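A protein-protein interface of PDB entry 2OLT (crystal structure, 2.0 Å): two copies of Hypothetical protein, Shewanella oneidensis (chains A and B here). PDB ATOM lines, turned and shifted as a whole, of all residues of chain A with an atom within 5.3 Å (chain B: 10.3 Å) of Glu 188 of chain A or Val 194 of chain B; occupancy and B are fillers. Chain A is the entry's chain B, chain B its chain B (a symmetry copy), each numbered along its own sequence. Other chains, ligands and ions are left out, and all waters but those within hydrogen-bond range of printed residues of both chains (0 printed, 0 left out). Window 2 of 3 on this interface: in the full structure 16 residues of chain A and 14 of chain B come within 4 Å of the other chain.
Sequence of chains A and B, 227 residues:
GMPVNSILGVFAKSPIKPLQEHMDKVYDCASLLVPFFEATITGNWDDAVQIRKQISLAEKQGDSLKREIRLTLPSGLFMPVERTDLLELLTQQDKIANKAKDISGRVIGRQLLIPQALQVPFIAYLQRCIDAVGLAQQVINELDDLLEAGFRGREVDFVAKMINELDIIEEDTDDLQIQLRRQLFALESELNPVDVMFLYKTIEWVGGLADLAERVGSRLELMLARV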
ATOM      1  N   LEU A 184      11.628 -20.429 -25.421  1.00  0.00           N
ATOM      2  CA  LEU A 184      10.744 -20.437 -24.254  1.00  0.00           C
ATOM      3  C   LEU A 184       9.740 -19.291 -24.364  1.00  0.00           C
ATOM      4  O   LEU A 184       8.543 -19.469 -24.124  1.00  0.00           O
ATOM      5  CB  LEU A 184      11.501 -20.311 -22.953  1.00  0.00           C
ATOM      6  CG  LEU A 184      10.695 -20.380 -21.641  1.00  0.00           C
ATOM      7  CD1 LEU A 184       9.764 -21.585 -21.586  1.00  0.00           C
ATOM      8  CD2 LEU A 184      11.675 -20.369 -20.466  1.00  0.00           C
ATOM      9  N   PHE A 185      10.209 -18.116 -24.764  1.00  0.00           N
ATOM     10  CA  PHE A 185       9.333 -16.963 -24.878  1.00  0.00           C
ATOM     11  C   PHE A 185       8.145 -17.276 -25.785  1.00  0.00           C
ATOM     12  O   PHE A 185       7.000 -16.878 -25.502  1.00  0.00           O
ATOM     13  CB  PHE A 185      10.113 -15.735 -25.397  1.00  0.00           C
ATOM     14  CG  PHE A 185       9.302 -14.477 -25.491  1.00  0.00           C
ATOM     15  CD1 PHE A 185       8.727 -13.921 -24.374  1.00  0.00           C
ATOM     16  CD2 PHE A 185       9.148 -13.820 -26.694  1.00  0.00           C
ATOM     17  CE1 PHE A 185       7.992 -12.783 -24.480  1.00  0.00           C
ATOM     18  CE2 PHE A 185       8.423 -12.665 -26.782  1.00  0.00           C
ATOM     19  CZ  PHE A 185       7.848 -12.147 -25.672  1.00  0.00           C
ATOM     20  N   ALA A 186       8.424 -17.981 -26.891  1.00  0.00           N
ATOM     21  CA  ALA A 186       7.394 -18.339 -27.846  1.00  0.00           C
ATOM     22  C   ALA A 186       6.389 -19.296 -27.236  1.00  0.00           C
ATOM     23  O   ALA A 186       5.244 -19.305 -27.629  1.00  0.00           O
ATOM     24  CB  ALA A 186       7.999 -18.944 -29.117  1.00  0.00           C
ATOM     25  N   LEU A 187       6.817 -20.099 -26.280  1.00  0.00           N
ATOM     26  CA  LEU A 187       5.941 -21.054 -25.653  1.00  0.00           C
ATOM     27  C   LEU A 187       5.220 -20.572 -24.415  1.00  0.00           C
ATOM     28  O   LEU A 187       4.325 -21.235 -23.950  1.00  0.00           O
ATOM     29  CB  LEU A 187       6.721 -22.257 -25.202  1.00  0.00           C
ATOM     30  CG  LEU A 187       7.277 -23.141 -26.294  1.00  0.00           C
ATOM     31  CD1 LEU A 187       8.006 -24.253 -25.552  1.00  0.00           C
ATOM     32  CD2 LEU A 187       6.155 -23.661 -27.191  1.00  0.00           C
ATOM     33  N   GLU A 188       5.627 -19.453 -23.841  1.00  0.00           N
ATOM     34  CA  GLU A 188       5.061 -19.021 -22.536  1.00  0.00           C
ATOM     35  C   GLU A 188       3.561 -19.068 -22.398  1.00  0.00           C
ATOM     36  O   GLU A 188       3.017 -19.334 -21.312  1.00  0.00           O
ATOM     37  CB  GLU A 188       5.432 -17.573 -22.187  1.00  0.00           C
ATOM     38  CG  GLU A 188       6.834 -17.393 -21.994  1.00  0.00           C
ATOM     39  CD  GLU A 188       7.222 -15.995 -21.588  1.00  0.00           C
ATOM     40  OE1 GLU A 188       6.372 -15.074 -21.395  1.00  0.00           O
ATOM     41  OE2 GLU A 188       8.438 -15.850 -21.503  1.00  0.00           O
ATOM     42  N   SER A 189       2.881 -18.720 -23.471  1.00  0.00           N
ATOM     43  CA  SER A 189       1.431 -18.688 -23.449  1.00  0.00           C
ATOM     44  C   SER A 189       0.808 -20.071 -23.299  1.00  0.00           C
ATOM     45  O   SER A 189      -0.364 -20.157 -22.986  1.00  0.00           O
ATOM     46  CB  SER A 189       0.868 -18.009 -24.707  1.00  0.00           C
ATOM     47  OG  SER A 189       1.073 -18.839 -25.847  1.00  0.00           O
ATOM     48  N   GLU A 190       1.565 -21.143 -23.518  1.00  0.00           N
ATOM     49  CA  GLU A 190       1.039 -22.478 -23.413  1.00  0.00           C
ATOM     50  C   GLU A 190       1.378 -23.114 -22.076  1.00  0.00           C
ATOM     51  O   GLU A 190       0.912 -24.217 -21.819  1.00  0.00           O
ATOM     52  CB  GLU A 190       1.578 -23.281 -24.587  1.00  0.00           C
ATOM     53  CG  GLU A 190       1.162 -22.663 -25.934  1.00  0.00           C
ATOM     54  CD  GLU A 190       1.784 -23.378 -27.135  1.00  0.00           C
ATOM     55  OE1 GLU A 190       2.168 -24.577 -26.989  1.00  0.00           O
ATOM     56  OE2 GLU A 190       1.899 -22.746 -28.228  1.00  0.00           O
ATOM     57  N   LEU A 191       2.101 -22.401 -21.192  1.00  0.00           N
ATOM     58  CA  LEU A 191       2.581 -22.990 -19.954  1.00  0.00           C
ATOM     59  C   LEU A 191       2.110 -22.226 -18.726  1.00  0.00           C
ATOM     60  O   LEU A 191       1.657 -21.100 -18.841  1.00  0.00           O
ATOM     61  CB  LEU A 191       4.109 -23.041 -20.039  1.00  0.00           C
ATOM     62  CG  LEU A 191       4.691 -23.697 -21.321  1.00  0.00           C
ATOM     63  CD1 LEU A 191       6.166 -23.458 -21.398  1.00  0.00           C
ATOM     64  CD2 LEU A 191       4.427 -25.213 -21.363  1.00  0.00           C
ATOM     65  N   ASN A 192       2.203 -22.861 -17.560  1.00  0.00           N
ATOM     66  CA  ASN A 192       1.848 -22.223 -16.284  1.00  0.00           C
ATOM     67  C   ASN A 192       2.922 -21.183 -15.984  1.00  0.00           C
ATOM     68  O   ASN A 192       4.101 -21.471 -16.163  1.00  0.00           O
ATOM     69  CB  ASN A 192       1.785 -23.264 -15.165  1.00  0.00           C
ATOM     70  CG  ASN A 192       1.454 -22.633 -13.777  1.00  0.00           C
ATOM     71  OD1 ASN A 192       2.339 -22.143 -13.049  1.00  0.00           O
ATOM     72  ND2 ASN A 192       0.162 -22.663 -13.414  1.00  0.00           N
ATOM     73  N   PRO A 193       2.516 -19.981 -15.537  1.00  0.00           N
ATOM     74  CA  PRO A 193       3.512 -18.935 -15.313  1.00  0.00           C
ATOM     75  C   PRO A 193       4.637 -19.250 -14.314  1.00  0.00           C
ATOM     76  O   PRO A 193       5.745 -18.813 -14.537  1.00  0.00           O
ATOM     77  CB  PRO A 193       2.664 -17.715 -14.913  1.00  0.00           C
ATOM     78  CG  PRO A 193       1.369 -18.285 -14.471  1.00  0.00           C
ATOM     79  CD  PRO A 193       1.159 -19.533 -15.235  1.00  0.00           C
ATOM     80  N   VAL A 196       7.076 -21.441 -16.036  1.00  0.00           N
ATOM     81  CA  VAL A 196       7.870 -20.646 -16.955  1.00  0.00           C
ATOM     82  C   VAL A 196       9.022 -20.002 -16.245  1.00  0.00           C
ATOM     83  O   VAL A 196      10.145 -20.092 -16.718  1.00  0.00           O
ATOM     84  CB  VAL A 196       7.004 -19.569 -17.656  1.00  0.00           C
ATOM     85  CG1 VAL A 196       7.879 -18.617 -18.409  1.00  0.00           C
ATOM     86  CG2 VAL A 196       6.025 -20.221 -18.585  1.00  0.00           C
ATOM     87  N   MET A 197       8.737 -19.314 -15.137  1.00  0.00           N
ATOM     88  CA  MET A 197       9.777 -18.659 -14.353  1.00  0.00           C
ATOM     89  C   MET A 197      10.850 -19.659 -13.909  1.00  0.00           C
ATOM     90  O   MET A 197      12.050 -19.368 -13.972  1.00  0.00           O
ATOM     91  CB  MET A 197       9.144 -17.974 -13.173  1.00  0.00           C
ATOM     92  CG  MET A 197       8.242 -16.864 -13.599  1.00  0.00           C
ATOM     93  SD  MET A 197       9.181 -15.595 -14.805  1.00  0.00           S
ATOM     94  CE  MET A 197      10.796 -15.277 -13.871  1.00  0.00           C
ATOM     95  N   TYR A 200      13.167 -20.307 -16.832  1.00  0.00           N
ATOM     96  CA  TYR A 200      14.134 -19.248 -16.948  1.00  0.00           C
ATOM     97  C   TYR A 200      15.194 -19.323 -15.846  1.00  0.00           C
ATOM     98  O   TYR A 200      16.373 -19.095 -16.140  1.00  0.00           O
ATOM     99  CB  TYR A 200      13.453 -17.860 -16.957  1.00  0.00           C
ATOM    100  CG  TYR A 200      12.778 -17.525 -18.250  1.00  0.00           C
ATOM    101  CD1 TYR A 200      13.511 -17.306 -19.401  1.00  0.00           C
ATOM    102  CD2 TYR A 200      11.388 -17.357 -18.318  1.00  0.00           C
ATOM    103  CE1 TYR A 200      12.874 -16.946 -20.617  1.00  0.00           C
ATOM    104  CE2 TYR A 200      10.762 -17.015 -19.479  1.00  0.00           C
ATOM    105  CZ  TYR A 200      11.497 -16.828 -20.644  1.00  0.00           C
ATOM    106  OH  TYR A 200      10.808 -16.485 -21.811  1.00  0.00           O
ATOM    107  N   ARG B 106      17.958  -8.845 -23.269  1.00  0.00           N
ATOM    108  CA  ARG B 106      16.727  -9.443 -22.750  1.00  0.00           C
ATOM    109  C   ARG B 106      15.522  -8.596 -23.172  1.00  0.00           C
ATOM    110  O   ARG B 106      14.439  -9.119 -23.501  1.00  0.00           O
ATOM    111  CB  ARG B 106      16.754  -9.541 -21.218  1.00  0.00           C
ATOM    112  CG  ARG B 106      17.857 -10.430 -20.619  1.00  0.00           C
ATOM    113  CD  ARG B 106      17.923 -11.798 -21.171  1.00  0.00           C
ATOM    114  NE  ARG B 106      16.714 -12.569 -20.947  1.00  0.00           N
ATOM    115  CZ  ARG B 106      16.481 -13.256 -19.835  1.00  0.00           C
ATOM    116  NH1 ARG B 106      17.328 -13.180 -18.832  1.00  0.00           N
ATOM    117  NH2 ARG B 106      15.377 -13.951 -19.687  1.00  0.00           N
ATOM    118  N   GLY B 109      14.783  -9.210 -26.732  1.00  0.00           N
ATOM    119  CA  GLY B 109      14.290 -10.572 -26.848  1.00  0.00           C
ATOM    120  C   GLY B 109      12.826 -10.750 -26.477  1.00  0.00           C
ATOM    121  O   GLY B 109      12.126 -11.555 -27.076  1.00  0.00           O
ATOM    122  N   ARG B 110      12.374 -10.031 -25.456  1.00  0.00           N
ATOM    123  CA  ARG B 110      10.988 -10.141 -25.011  1.00  0.00           C
ATOM    124  C   ARG B 110      10.153  -8.969 -25.543  1.00  0.00           C
ATOM    125  O   ARG B 110       8.950  -8.929 -25.310  1.00  0.00           O
ATOM    126  CB  ARG B 110      10.918 -10.103 -23.468  1.00  0.00           C
ATOM    127  CG  ARG B 110      11.686 -11.244 -22.786  1.00  0.00           C
ATOM    128  CD  ARG B 110      11.410 -11.361 -21.277  1.00  0.00           C
ATOM    129  NE  ARG B 110       9.975 -11.384 -20.965  1.00  0.00           N
ATOM    130  CZ  ARG B 110       9.204 -12.467 -20.910  1.00  0.00           C
ATOM    131  NH1 ARG B 110       9.716 -13.658 -21.132  1.00  0.00           N
ATOM    132  NH2 ARG B 110       7.887 -12.356 -20.648  1.00  0.00           N
ATOM    133  N   GLN B 111      10.778  -8.077 -26.310  1.00  0.00           N
ATOM    134  CA  GLN B 111      10.165  -6.801 -26.681  1.00  0.00           C
ATOM    135  C   GLN B 111       9.474  -6.251 -25.429  1.00  0.00           C
ATOM    136  O   GLN B 111       8.290  -5.947 -25.422  1.00  0.00           O
ATOM    137  CB  GLN B 111       9.178  -6.895 -27.857  1.00  0.00           C
ATOM    138  CG  GLN B 111       9.834  -6.929 -29.227  1.00  0.00           C
ATOM    139  CD  GLN B 111       8.999  -6.229 -30.306  1.00  0.00           C
ATOM    140  OE1 GLN B 111       7.751  -6.166 -30.247  1.00  0.00           O
ATOM    141  NE2 GLN B 111       9.694  -5.662 -31.283  1.00  0.00           N
ATOM    142  N   LEU B 112      10.227  -6.150 -24.345  1.00  0.00           N
ATOM    143  CA  LEU B 112       9.660  -5.806 -23.064  1.00  0.00           C
ATOM    144  C   LEU B 112       9.214  -4.369 -23.063  1.00  0.00           C
ATOM    145  O   LEU B 112      10.016  -3.465 -23.257  1.00  0.00           O
ATOM    146  CB  LEU B 112      10.678  -6.064 -21.950  1.00  0.00           C
ATOM    147  CG  LEU B 112      10.356  -5.844 -20.464  1.00  0.00           C
ATOM    148  CD1 LEU B 112      11.232  -6.805 -19.560  1.00  0.00           C
ATOM    149  CD2 LEU B 112      10.573  -4.361 -20.139  1.00  0.00           C
ATOM    150  N   LEU B 113       7.921  -4.192 -22.812  1.00  0.00           N
ATOM    151  CA  LEU B 113       7.269  -2.890 -22.684  1.00  0.00           C
ATOM    152  C   LEU B 113       7.103  -2.409 -21.243  1.00  0.00           C
ATOM    153  O   LEU B 113       6.475  -3.072 -20.437  1.00  0.00           O
ATOM    154  CB  LEU B 113       5.835  -3.028 -23.199  1.00  0.00           C
ATOM    155  CG  LEU B 113       5.538  -3.566 -24.600  1.00  0.00           C
ATOM    156  N   LEU B 184       4.444  -0.637  -9.597  1.00  0.00           N
ATOM    157  CA  LEU B 184       4.246  -1.912 -10.288  1.00  0.00           C
ATOM    158  C   LEU B 184       3.297  -2.793  -9.477  1.00  0.00           C
ATOM    159  O   LEU B 184       2.376  -3.404 -10.023  1.00  0.00           O
ATOM    160  CB  LEU B 184       5.542  -2.654 -10.515  1.00  0.00           C
ATOM    161  CG  LEU B 184       5.484  -3.981 -11.300  1.00  0.00           C
ATOM    162  CD1 LEU B 184       4.722  -3.854 -12.613  1.00  0.00           C
ATOM    163  CD2 LEU B 184       6.915  -4.477 -11.523  1.00  0.00           C
ATOM    164  N   GLU B 188      -0.027  -4.873 -10.834  1.00  0.00           N
ATOM    165  CA  GLU B 188       0.113  -6.326 -11.113  1.00  0.00           C
ATOM    166  C   GLU B 188      -1.126  -7.050 -11.577  1.00  0.00           C
ATOM    167  O   GLU B 188      -1.063  -7.997 -12.380  1.00  0.00           O
ATOM    168  CB  GLU B 188       0.582  -7.117  -9.885  1.00  0.00           C
ATOM    169  CG  GLU B 188       1.895  -6.755  -9.463  1.00  0.00           C
ATOM    170  CD  GLU B 188       2.407  -7.559  -8.297  1.00  0.00           C
ATOM    171  OE1 GLU B 188       1.745  -8.504  -7.769  1.00  0.00           O
ATOM    172  OE2 GLU B 188       3.506  -7.175  -7.906  1.00  0.00           O
ATOM    173  N   GLU B 190      -3.378  -6.059 -13.445  1.00  0.00           N
ATOM    174  CA  GLU B 190      -3.762  -5.737 -14.794  1.00  0.00           C
ATOM    175  C   GLU B 190      -2.800  -6.329 -15.810  1.00  0.00           C
ATOM    176  O   GLU B 190      -3.060  -6.208 -17.001  1.00  0.00           O
ATOM    177  CB  GLU B 190      -3.854  -4.223 -14.900  1.00  0.00           C
ATOM    178  CG  GLU B 190      -4.888  -3.649 -13.915  1.00  0.00           C
ATOM    179  CD  GLU B 190      -4.922  -2.119 -13.911  1.00  0.00           C
ATOM    180  OE1 GLU B 190      -4.495  -1.506 -14.935  1.00  0.00           O
ATOM    181  OE2 GLU B 190      -5.369  -1.522 -12.886  1.00  0.00           O
ATOM    182  N   LEU B 191      -1.749  -7.040 -15.359  1.00  0.00           N
ATOM    183  CA  LEU B 191      -0.713  -7.516 -16.259  1.00  0.00           C
ATOM    184  C   LEU B 191      -0.534  -9.024 -16.193  1.00  0.00           C
ATOM    185  O   LEU B 191      -1.005  -9.657 -15.264  1.00  0.00           O
ATOM    186  CB  LEU B 191       0.577  -6.775 -15.897  1.00  0.00           C
ATOM    187  CG  LEU B 191       0.468  -5.228 -15.820  1.00  0.00           C
ATOM    188  CD1 LEU B 191       1.711  -4.652 -15.218  1.00  0.00           C
ATOM    189  CD2 LEU B 191       0.243  -4.596 -17.206  1.00  0.00           C
ATOM    190  N   ASN B 192       0.130  -9.589 -17.199  1.00  0.00           N
ATOM    191  CA  ASN B 192       0.435 -11.026 -17.235  1.00  0.00           C
ATOM    192  C   ASN B 192       1.500 -11.289 -16.175  1.00  0.00           C
ATOM    193  O   ASN B 192       2.444 -10.513 -16.071  1.00  0.00           O
ATOM    194  CB  ASN B 192       0.947 -11.430 -18.619  1.00  0.00           C
ATOM    195  CG  ASN B 192       1.329 -12.940 -18.701  1.00  0.00           C
ATOM    196  OD1 ASN B 192       2.448 -13.357 -18.344  1.00  0.00           O
ATOM    197  ND2 ASN B 192       0.381 -13.757 -19.187  1.00  0.00           N
ATOM    198  N   PRO B 193       1.344 -12.372 -15.394  1.00  0.00           N
ATOM    199  CA  PRO B 193       2.304 -12.612 -14.318  1.00  0.00           C
ATOM    200  C   PRO B 193       3.779 -12.758 -14.723  1.00  0.00           C
ATOM    201  O   PRO B 193       4.628 -12.319 -13.977  1.00  0.00           O
ATOM    202  CB  PRO B 193       1.740 -13.855 -13.609  1.00  0.00           C
ATOM    203  CG  PRO B 193       0.838 -14.481 -14.605  1.00  0.00           C
ATOM    204  CD  PRO B 193       0.302 -13.394 -15.450  1.00  0.00           C
ATOM    205  N   VAL B 194       4.079 -13.364 -15.876  1.00  0.00           N
ATOM    206  CA  VAL B 194       5.465 -13.493 -16.325  1.00  0.00           C
ATOM    207  C   VAL B 194       6.017 -12.096 -16.683  1.00  0.00           C
ATOM    208  O   VAL B 194       7.142 -11.724 -16.354  1.00  0.00           O
ATOM    209  CB  VAL B 194       5.571 -14.491 -17.517  1.00  0.00           C
ATOM    210  CG1 VAL B 194       7.004 -14.569 -18.030  1.00  0.00           C
ATOM    211  CG2 VAL B 194       5.095 -15.865 -17.088  1.00  0.00           C
ATOM    212  N   ASP B 195       5.201 -11.305 -17.351  1.00  0.00           N
ATOM    213  CA  ASP B 195       5.588  -9.941 -17.670  1.00  0.00           C
ATOM    214  C   ASP B 195       5.901  -9.155 -16.394  1.00  0.00           C
ATOM    215  O   ASP B 195       6.845  -8.384 -16.328  1.00  0.00           O
ATOM    216  CB  ASP B 195       4.468  -9.207 -18.437  1.00  0.00           C
ATOM    217  CG  ASP B 195       4.223  -9.743 -19.868  1.00  0.00           C
ATOM    218  OD1 ASP B 195       5.088 -10.491 -20.409  1.00  0.00           O
ATOM    219  OD2 ASP B 195       3.139  -9.376 -20.445  1.00  0.00           O
ATOM    220  N   VAL B 196       5.099  -9.358 -15.370  1.00  0.00           N
ATOM    221  CA  VAL B 196       5.326  -8.682 -14.106  1.00  0.00           C
ATOM    222  C   VAL B 196       6.666  -9.044 -13.541  1.00  0.00           C
ATOM    223  O   VAL B 196       7.415  -8.158 -13.158  1.00  0.00           O
ATOM    224  CB  VAL B 196       4.209  -9.015 -13.085  1.00  0.00           C
ATOM    225  CG1 VAL B 196       4.585  -8.508 -11.729  1.00  0.00           C
ATOM    226  CG2 VAL B 196       2.911  -8.408 -13.525  1.00  0.00           C
ATOM    227  N   MET B 197       6.950 -10.345 -13.449  1.00  0.00           N
ATOM    228  CA  MET B 197       8.228 -10.815 -12.932  1.00  0.00           C
ATOM    229  C   MET B 197       9.398 -10.233 -13.731  1.00  0.00           C
ATOM    230  O   MET B 197      10.409  -9.810 -13.158  1.00  0.00           O
ATOM    231  CB  MET B 197       8.244 -12.320 -12.956  1.00  0.00           C
ATOM    232  CG  MET B 197       7.230 -12.896 -12.025  1.00  0.00           C
ATOM    233  SD  MET B 197       7.434 -12.159 -10.191  1.00  0.00           S
ATOM    234  CE  MET B 197       9.293 -12.343  -9.892  1.00  0.00           C
ATOM    235  N   PHE B 198       9.262 -10.181 -15.046  1.00  0.00           N
ATOM    236  CA  PHE B 198      10.330  -9.567 -15.858  1.00  0.00           C
ATOM    237  C   PHE B 198      10.512  -8.076 -15.646  1.00  0.00           C
ATOM    238  O   PHE B 198      11.637  -7.561 -15.714  1.00  0.00           O
ATOM    239  CB  PHE B 198      10.306  -9.997 -17.313  1.00  0.00           C
ATOM    240  CG  PHE B 198      10.969 -11.321 -17.494  1.00  0.00           C
ATOM    241  CD1 PHE B 198      12.365 -11.434 -17.432  1.00  0.00           C
ATOM    242  CD2 PHE B 198      10.232 -12.480 -17.599  1.00  0.00           C
ATOM    243  CE1 PHE B 198      13.003 -12.711 -17.512  1.00  0.00           C
ATOM    244  CE2 PHE B 198      10.867 -13.736 -17.697  1.00  0.00           C
ATOM    245  CZ  PHE B 198      12.242 -13.840 -17.661  1.00  0.00           C
ATOM    246  N   LEU B 199       9.435  -7.396 -15.293  1.00  0.00           N
ATOM    247  CA  LEU B 199       9.545  -6.006 -14.912  1.00  0.00           C
ATOM    248  C   LEU B 199      10.319  -5.863 -13.576  1.00  0.00           C
ATOM    249  O   LEU B 199      11.190  -4.991 -13.461  1.00  0.00           O
ATOM    250  CB  LEU B 199       8.167  -5.364 -14.863  1.00  0.00           C
ATOM    251  CG  LEU B 199       7.535  -5.012 -16.225  1.00  0.00           C
ATOM    252  CD1 LEU B 199       6.070  -4.676 -16.093  1.00  0.00           C
ATOM    253  CD2 LEU B 199       8.292  -3.833 -16.864  1.00  0.00           C
ATOM    254  N   TYR B 200       9.995  -6.682 -12.565  1.00  0.00           N
ATOM    255  CA  TYR B 200      10.763  -6.676 -11.348  1.00  0.00           C
ATOM    256  C   TYR B 200      12.228  -7.042 -11.598  1.00  0.00           C
ATOM    257  O   TYR B 200      13.106  -6.420 -10.990  1.00  0.00           O
ATOM    258  CB  TYR B 200      10.140  -7.612 -10.284  1.00  0.00           C
ATOM    259  CG  TYR B 200       8.912  -7.056  -9.635  1.00  0.00           C
ATOM    260  CD1 TYR B 200       8.983  -5.958  -8.799  1.00  0.00           C
ATOM    261  CD2 TYR B 200       7.665  -7.675  -9.797  1.00  0.00           C
ATOM    262  CE1 TYR B 200       7.825  -5.456  -8.149  1.00  0.00           C
ATOM    263  CE2 TYR B 200       6.544  -7.204  -9.182  1.00  0.00           C
ATOM    264  CZ  TYR B 200       6.610  -6.079  -8.369  1.00  0.00           C
ATOM    265  OH  TYR B 200       5.431  -5.630  -7.766  1.00  0.00           O
ATOM    266  N   LYS B 201      12.499  -8.060 -12.437  1.00  0.00           N
ATOM    267  CA  LYS B 201      13.855  -8.445 -12.765  1.00  0.00           C
ATOM    268  C   LYS B 201      14.609  -7.293 -13.432  1.00  0.00           C
ATOM    269  O   LYS B 201      15.782  -7.093 -13.167  1.00  0.00           O
ATOM    270  CB  LYS B 201      13.931  -9.698 -13.652  1.00  0.00           C
ATOM    271  CG  LYS B 201      13.369 -10.971 -12.982  1.00  0.00           C
ATOM    272  CD  LYS B 201      14.101 -12.279 -13.454  1.00  0.00           C
ATOM    273  CE  LYS B 201      15.281 -12.695 -12.491  1.00  0.00           C
ATOM    274  NZ  LYS B 201      16.234 -11.596 -12.062  1.00  0.00           N
ATOM    275  N   THR B 202      13.945  -6.569 -14.322  1.00  0.00           N
ATOM    276  CA  THR B 202      14.570  -5.446 -15.002  1.00  0.00           C
ATOM    277  C   THR B 202      14.977  -4.361 -13.996  1.00  0.00           C
ATOM    278  O   THR B 202      16.079  -3.817 -14.065  1.00  0.00           O
ATOM    279  CB  THR B 202      13.673  -4.900 -16.150  1.00  0.00           C
ATOM    280  OG1 THR B 202      13.492  -5.937 -17.129  1.00  0.00           O
ATOM    281  CG2 THR B 202      14.326  -3.744 -16.815  1.00  0.00           C
ATOM    282  N   TRP B 205      18.015  -5.696 -12.226  1.00  0.00           N
ATOM    283  CA  TRP B 205      19.200  -5.689 -13.050  1.00  0.00           C
ATOM    284  C   TRP B 205      19.792  -4.289 -13.151  1.00  0.00           C
ATOM    285  O   TRP B 205      21.011  -4.127 -13.107  1.00  0.00           O
ATOM    286  CB  TRP B 205      18.941  -6.208 -14.458  1.00  0.00           C
ATOM    287  CG  TRP B 205      18.543  -7.656 -14.568  1.00  0.00           C
ATOM    288  CD1 TRP B 205      18.982  -8.708 -13.810  1.00  0.00           C
ATOM    289  CD2 TRP B 205      17.722  -8.223 -15.597  1.00  0.00           C
ATOM    290  NE1 TRP B 205      18.438  -9.879 -14.271  1.00  0.00           N
ATOM    291  CE2 TRP B 205      17.669  -9.602 -15.379  1.00  0.00           C
ATOM    292  CE3 TRP B 205      17.005  -7.686 -16.665  1.00  0.00           C
ATOM    293  CZ2 TRP B 205      16.915 -10.449 -16.182  1.00  0.00           C
ATOM    294  CZ3 TRP B 205      16.282  -8.540 -17.485  1.00  0.00           C
ATOM    295  CH2 TRP B 205      16.220  -9.896 -17.214  1.00  0.00           C
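The guanidinium group of Arg 110 of chain B sits at hydrogen-bond distance from the side-chain hydroxyl of Tyr 200 of chain A, at 3.1 Å.
The side-chain carboxylate (OE2) of Glu 188 of chain A is in salt-bridge range of the guanidinium group (NH1) of Arg 110 of chain B, 2.6 Å away.
The side-chain carboxylate (OE2) of Glu 188 of chain A lies within hydrogen-bond range of the side-chain hydroxyl (OH) of Tyr 200 of chain A (2.5 Å).
The backbone NH (N) of Val 194 of chain B lies within hydrogen-bond range of the side-chain amide oxygen (OD1) of Asn 192 of chain B (3.0 Å).
The backbone carbonyl oxygen (O) of Phe 198 of chain B sits at hydrogen-bond distance from the side-chain hydroxyl (OG1) of Thr 202 of chain B (2.8 Å).
The guanidinium group (NH2) of Arg 110 of chain B is in salt-bridge range of the side-chain carboxylate (OD1) of Asp 195 of chain B (3.4 Å).
Phe 185 of chain A touches Gly 109 of chain B.
NH1 of Arg 110 of chain B touches CD1 of Phe 185 of chain A, 3.4 Å away.
Glu 188 of chain A touches Val 194 of chain B (OE1 to CG1, 3.5 Å).
CG of Pro 193 of chain B touches CB of Pro 193 of chain A (3.7 Å).
CB of Pro 193 of chain A touches CG2 of Val 194 of chain B, 3.8 Å away.
Met 197 of chain B touches Met 197 of chain A (CB to SD, 3.9 Å).
Met 197 of chain A touches Phe 198 of chain B (SD to CE2, 3.8 Å).
Tyr 200 of chain A touches Arg 106 of chain B (CD1 to NH2, 3.8 Å).
Phe 198 of chain B touches Tyr 200 of chain A (CZ to CD2, 3.7 Å).
Phe 185 of chain A touches just these residues of chain B: Gly 109 (3.8 Å) and Arg 110 (3.4 Å).
Glu 188 of chain A touches just these residues of chain B: Arg 110 (2.6 Å) and Val 194 (3.5 Å).
No residue of chain B comes within 4 Å of Ser 189 of chain A.
Leu 191 of chain A touches none of the printed residues of chain B.
Pro 193 of chain A touches just these residues of chain B: Pro 193 (3.7 Å) and Val 194 (3.8 Å).
Printed residues of chain B within 4 Å of Tyr 200 of chain A: Arg 106, Arg 110 and Phe 198.
Of the printed residues of chain A, Arg 110 of chain B touches Phe 185 (3.4 Å), Glu 188 (2.6 Å) and Tyr 200 (3.1 Å).
Leu 112 of chain B touches none of the printed residues of chain A.
Printed residues of chain A within 4 Å of Pro 193 of chain B: Pro 193 (3.7 Å).
Of chain A, only Glu 188 (3.5 Å) and Pro 193 (3.8 Å) come within 4 Å of Val 194 of chain B.
Printed residues of chain A within 4 Å of Met 197 of chain B: Met 197.
The nearest residue of chain B that does not touch Glu 188 of chain A is Asp 195 of chain B (4.9 Å).
The nearest residue of chain A that does not touch Val 194 of chain B is Met 197 of chain A (4.02 Å).
Of the 22 printed residues of chain B, 7 touch a printed residue of chain A.
Printed residues of chain B that touch a printed residue of chain A: Arg 106, Gly 109, Arg 110, Pro 193, Val 194, Met 197 and Phe 198.
Hydrophobic or aromatic side chains of chain B that line the printed part of chain A: Pro 193, Val 194, Met 197 and Phe 198.
Among the printed residues, 11 pairs touch across the chains.
Among the printed residues, Asp or Glu carboxylates within 4 Å of a Lys or Arg side-chain nitrogen of the other chain: Glu 188 of chain A with Arg 110 of chain B (2.6 Å).
Pro 193 of chain A touches its own counterpart, Pro 193 of chain B.
Met 197 of chain B touches its own counterpart, Met 197 of chain A.
Positions printed for both chains: 184, 188, 190, 191, 192, 193, 196, 197 and 200.
Of the 11 pairs that touch across the chains among the printed residues, 2 have their exchanged pair printed and touching as well.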
